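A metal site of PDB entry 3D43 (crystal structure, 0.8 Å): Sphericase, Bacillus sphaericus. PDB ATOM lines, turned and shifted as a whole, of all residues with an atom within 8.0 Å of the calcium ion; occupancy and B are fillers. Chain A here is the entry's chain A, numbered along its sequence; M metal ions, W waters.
The backbone NH (N) of Asp 217 lies within hydrogen-bond range of the side-chain carboxylate (OD1) of Asp 298, 3.3 Å away.
Of the 17 residues printed, 5 come within 4 Å of the calcium ion.
O of Thr 214 is bound to the calcium ion.
The calcium ion is bound by O of Val 219.
OD1 of Asp 224 binds the calcium ion.
The side-chain amide oxygen (OE1) of Gln 221 is bound to the calcium ion (2.3 Å).
The calcium ion is bound by water W1 (2.3 Å).
OD2 of Asp 217 is bound to the calcium ion, at 2.4 Å.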
ATOM      1  N   TYR A 211     -32.527  25.509   3.842  1.00  0.00           N
ATOM      2  CA  TYR A 211     -31.443  26.430   4.120  1.00  0.00           C
ATOM      3  C   TYR A 211     -30.410  26.418   2.999  1.00  0.00           C
ATOM      4  O   TYR A 211     -30.031  25.402   2.446  1.00  0.00           O
ATOM      5  CB  TYR A 211     -30.766  26.062   5.426  1.00  0.00           C
ATOM      6  CG  TYR A 211     -31.673  26.203   6.616  1.00  0.00           C
ATOM      7  CD1 TYR A 211     -32.499  25.140   7.010  1.00  0.00           C
ATOM      8  CD2 TYR A 211     -31.738  27.384   7.347  1.00  0.00           C
ATOM      9  CE1 TYR A 211     -33.337  25.271   8.113  1.00  0.00           C
ATOM     10  CE2 TYR A 211     -32.571  27.493   8.445  1.00  0.00           C
ATOM     11  CZ  TYR A 211     -33.380  26.452   8.823  1.00  0.00           C
ATOM     12  OH  TYR A 211     -34.197  26.617   9.921  1.00  0.00           O
ATOM     13  N   ILE A 212     -29.886  27.617   2.635  1.00  0.00           N
ATOM     14  CA  ILE A 212     -28.872  27.716   1.624  1.00  0.00           C
ATOM     15  C   ILE A 212     -27.641  26.903   1.950  1.00  0.00           C
ATOM     16  O   ILE A 212     -27.078  26.243   1.049  1.00  0.00           O
ATOM     17  CB  ILE A 212     -28.541  29.182   1.410  1.00  0.00           C
ATOM     18  CG1 ILE A 212     -29.679  29.867   0.655  1.00  0.00           C
ATOM     19  CG2 ILE A 212     -27.213  29.405   0.715  1.00  0.00           C
ATOM     20  CD1 ILE A 212     -29.619  31.372   0.577  1.00  0.00           C
ATOM     21  N   SER A 213     -27.133  27.002   3.156  1.00  0.00           N
ATOM     22  CA  SER A 213     -25.787  26.456   3.363  1.00  0.00           C
ATOM     23  C   SER A 213     -25.656  24.961   3.071  1.00  0.00           C
ATOM     24  O   SER A 213     -24.614  24.577   2.574  1.00  0.00           O
ATOM     25  CB  SER A 213     -25.465  26.707   4.823  1.00  0.00           C
ATOM     26  OG  SER A 213     -26.342  26.013   5.713  1.00  0.00           O
ATOM     27  N   THR A 214     -26.712  24.194   3.404  1.00  0.00           N
ATOM     28  CA  THR A 214     -26.605  22.760   3.229  1.00  0.00           C
ATOM     29  C   THR A 214     -27.307  22.263   1.985  1.00  0.00           C
ATOM     30  O   THR A 214     -27.279  21.055   1.729  1.00  0.00           O
ATOM     31  CB  THR A 214     -27.148  22.055   4.487  1.00  0.00           C
ATOM     32  OG1 THR A 214     -28.495  22.514   4.677  1.00  0.00           O
ATOM     33  CG2 THR A 214     -26.313  22.404   5.721  1.00  0.00           C
ATOM     34  N   ALA A 215     -27.924  23.113   1.194  1.00  0.00           N
ATOM     35  CA  ALA A 215     -28.495  22.704  -0.088  1.00  0.00           C
ATOM     36  C   ALA A 215     -27.366  22.570  -1.111  1.00  0.00           C
ATOM     37  O   ALA A 215     -26.406  23.324  -1.018  1.00  0.00           O
ATOM     38  CB  ALA A 215     -29.543  23.697  -0.549  1.00  0.00           C
ATOM     39  N   GLY A 216     -27.522  21.695  -2.071  1.00  0.00           N
ATOM     40  CA  GLY A 216     -26.748  21.603  -3.250  1.00  0.00           C
ATOM     41  C   GLY A 216     -25.890  20.427  -3.453  1.00  0.00           C
ATOM     42  O   GLY A 216     -25.453  20.128  -4.563  1.00  0.00           O
ATOM     43  N   ASP A 217     -25.657  19.673  -2.380  1.00  0.00           N
ATOM     44  CA  ASP A 217     -24.759  18.539  -2.375  1.00  0.00           C
ATOM     45  C   ASP A 217     -25.461  17.202  -2.630  1.00  0.00           C
ATOM     46  O   ASP A 217     -24.758  16.190  -2.667  1.00  0.00           O
ATOM     47  CB  ASP A 217     -24.005  18.477  -1.044  1.00  0.00           C
ATOM     48  CG  ASP A 217     -24.848  18.316   0.213  1.00  0.00           C
ATOM     49  OD1 ASP A 217     -24.259  17.998   1.268  1.00  0.00           O
ATOM     50  OD2 ASP A 217     -26.065  18.581   0.114  1.00  0.00           O
ATOM     51  N   TYR A 218     -26.782  17.170  -2.763  1.00  0.00           N
ATOM     52  CA  TYR A 218     -27.508  15.895  -2.901  1.00  0.00           C
ATOM     53  C   TYR A 218     -27.185  14.945  -1.760  1.00  0.00           C
ATOM     54  O   TYR A 218     -27.184  13.720  -1.973  1.00  0.00           O
ATOM     55  CB  TYR A 218     -27.276  15.293  -4.287  1.00  0.00           C
ATOM     56  CG  TYR A 218     -27.914  15.953  -5.465  1.00  0.00           C
ATOM     57  CD1 TYR A 218     -27.108  16.737  -6.291  1.00  0.00           C
ATOM     58  CD2 TYR A 218     -29.249  15.843  -5.745  1.00  0.00           C
ATOM     59  CE1 TYR A 218     -27.657  17.377  -7.390  1.00  0.00           C
ATOM     60  CE2 TYR A 218     -29.795  16.457  -6.871  1.00  0.00           C
ATOM     61  CZ  TYR A 218     -29.008  17.234  -7.688  1.00  0.00           C
ATOM     62  OH  TYR A 218     -29.528  17.824  -8.807  1.00  0.00           O
ATOM     63  N   VAL A 219     -26.997  15.476  -0.559  1.00  0.00           N
ATOM     64  CA  VAL A 219     -26.861  14.678   0.661  1.00  0.00           C
ATOM     65  C   VAL A 219     -27.703  15.332   1.719  1.00  0.00           C
ATOM     66  O   VAL A 219     -27.581  16.536   1.929  1.00  0.00           O
ATOM     67  CB  VAL A 219     -25.395  14.562   1.141  1.00  0.00           C
ATOM     68  CG1 VAL A 219     -25.345  13.776   2.445  1.00  0.00           C
ATOM     69  CG2 VAL A 219     -24.570  13.861   0.064  1.00  0.00           C
ATOM     70  N   ILE A 220     -28.579  14.610   2.385  1.00  0.00           N
ATOM     71  CA  ILE A 220     -29.502  15.237   3.331  1.00  0.00           C
ATOM     72  C   ILE A 220     -28.924  15.414   4.725  1.00  0.00           C
ATOM     73  O   ILE A 220     -28.579  14.478   5.395  1.00  0.00           O
ATOM     74  CB  ILE A 220     -30.814  14.406   3.440  1.00  0.00           C
ATOM     75  CG1 ILE A 220     -31.543  14.362   2.085  1.00  0.00           C
ATOM     76  CG2 ILE A 220     -31.708  14.930   4.560  1.00  0.00           C
ATOM     77  CD1 ILE A 220     -32.123  15.695   1.655  1.00  0.00           C
ATOM     78  N   GLN A 221     -28.846  16.698   5.096  1.00  0.00           N
ATOM     79  CA  GLN A 221     -28.560  17.124   6.451  1.00  0.00           C
ATOM     80  C   GLN A 221     -29.855  17.645   7.088  1.00  0.00           C
ATOM     81  O   GLN A 221     -30.873  17.837   6.429  1.00  0.00           O
ATOM     82  CB  GLN A 221     -27.476  18.205   6.462  1.00  0.00           C
ATOM     83  CG  GLN A 221     -26.123  17.696   6.043  1.00  0.00           C
ATOM     84  CD  GLN A 221     -25.875  17.841   4.563  1.00  0.00           C
ATOM     85  OE1 GLN A 221     -26.441  18.686   3.870  1.00  0.00           O
ATOM     86  NE2 GLN A 221     -24.976  17.021   4.022  1.00  0.00           N
ATOM     87  N   GLU A 222     -29.773  17.929   8.406  1.00  0.00           N
ATOM     88  CA  GLU A 222     -30.891  18.564   9.088  1.00  0.00           C
ATOM     89  C   GLU A 222     -31.253  19.858   8.402  1.00  0.00           C
ATOM     90  O   GLU A 222     -30.328  20.645   8.085  1.00  0.00           O
ATOM     91  CB  GLU A 222     -30.516  18.804  10.546  1.00  0.00           C
ATOM     92  CG  GLU A 222     -31.647  19.411  11.374  1.00  0.00           C
ATOM     93  CD  GLU A 222     -31.382  19.469  12.870  1.00  0.00           C
ATOM     94  OE1 GLU A 222     -32.176  20.133  13.565  1.00  0.00           O
ATOM     95  OE2 GLU A 222     -30.473  18.829  13.369  1.00  0.00           O
ATOM     96  N   GLY A 223     -32.524  20.098   8.147  1.00  0.00           N
ATOM     97  CA  GLY A 223     -32.993  21.301   7.519  1.00  0.00           C
ATOM     98  C   GLY A 223     -33.163  21.232   6.013  1.00  0.00           C
ATOM     99  O   GLY A 223     -33.637  22.218   5.416  1.00  0.00           O
ATOM    100  N   ASP A 224     -32.806  20.134   5.360  1.00  0.00           N
ATOM    101  CA  ASP A 224     -32.905  20.017   3.926  1.00  0.00           C
ATOM    102  C   ASP A 224     -34.235  19.426   3.466  1.00  0.00           C
ATOM    103  O   ASP A 224     -34.733  18.411   3.985  1.00  0.00           O
ATOM    104  CB  ASP A 224     -31.815  19.091   3.420  1.00  0.00           C
ATOM    105  CG  ASP A 224     -30.399  19.628   3.483  1.00  0.00           C
ATOM    106  OD1 ASP A 224     -29.462  18.833   3.269  1.00  0.00           O
ATOM    107  OD2 ASP A 224     -30.241  20.838   3.689  1.00  0.00           O
ATOM    108  N   ILE A 225     -34.767  20.087   2.439  1.00  0.00           N
ATOM    109  CA  ILE A 225     -35.872  19.514   1.650  1.00  0.00           C
ATOM    110  C   ILE A 225     -35.326  18.377   0.832  1.00  0.00           C
ATOM    111  O   ILE A 225     -34.173  18.440   0.361  1.00  0.00           O
ATOM    112  CB  ILE A 225     -36.451  20.612   0.762  1.00  0.00           C
ATOM    113  CG1 ILE A 225     -36.930  21.836   1.517  1.00  0.00           C
ATOM    114  CG2 ILE A 225     -37.530  20.066  -0.179  1.00  0.00           C
ATOM    115  CD1 ILE A 225     -38.188  21.612   2.334  1.00  0.00           C
ATOM    116  N   ASP A 298     -29.850  20.442  -6.778  1.00  0.00           N
ATOM    117  CA  ASP A 298     -30.465  20.299  -5.477  1.00  0.00           C
ATOM    118  C   ASP A 298     -30.600  21.695  -4.876  1.00  0.00           C
ATOM    119  O   ASP A 298     -29.624  22.419  -4.782  1.00  0.00           O
ATOM    120  CB  ASP A 298     -29.531  19.409  -4.600  1.00  0.00           C
ATOM    121  CG  ASP A 298     -29.861  19.315  -3.165  1.00  0.00           C
ATOM    122  OD1 ASP A 298     -28.896  19.092  -2.366  1.00  0.00           O
ATOM    123  OD2 ASP A 298     -31.047  19.465  -2.809  1.00  0.00           O
ATOM    124  N   PHE A 304     -34.078  17.572  -4.033  1.00  0.00           N
ATOM    125  CA  PHE A 304     -33.391  16.898  -5.090  1.00  0.00           C
ATOM    126  C   PHE A 304     -34.190  16.981  -6.398  1.00  0.00           C
ATOM    127  O   PHE A 304     -33.558  16.880  -7.461  1.00  0.00           O
ATOM    128  CB  PHE A 304     -33.173  15.422  -4.736  1.00  0.00           C
ATOM    129  CG  PHE A 304     -32.163  15.161  -3.641  1.00  0.00           C
ATOM    130  CD1 PHE A 304     -31.696  16.140  -2.752  1.00  0.00           C
ATOM    131  CD2 PHE A 304     -31.694  13.873  -3.464  1.00  0.00           C
ATOM    132  CE1 PHE A 304     -30.842  15.809  -1.729  1.00  0.00           C
ATOM    133  CE2 PHE A 304     -30.811  13.530  -2.477  1.00  0.00           C
ATOM    134  CZ  PHE A 304     -30.417  14.511  -1.577  1.00  0.00           C
HETATM  135 CA    CA M   1     -27.614  18.820   1.875  1.00  0.00          CA
HETATM  136  O   HOH W   1     -29.272  18.822   0.223  1.00  0.00           O
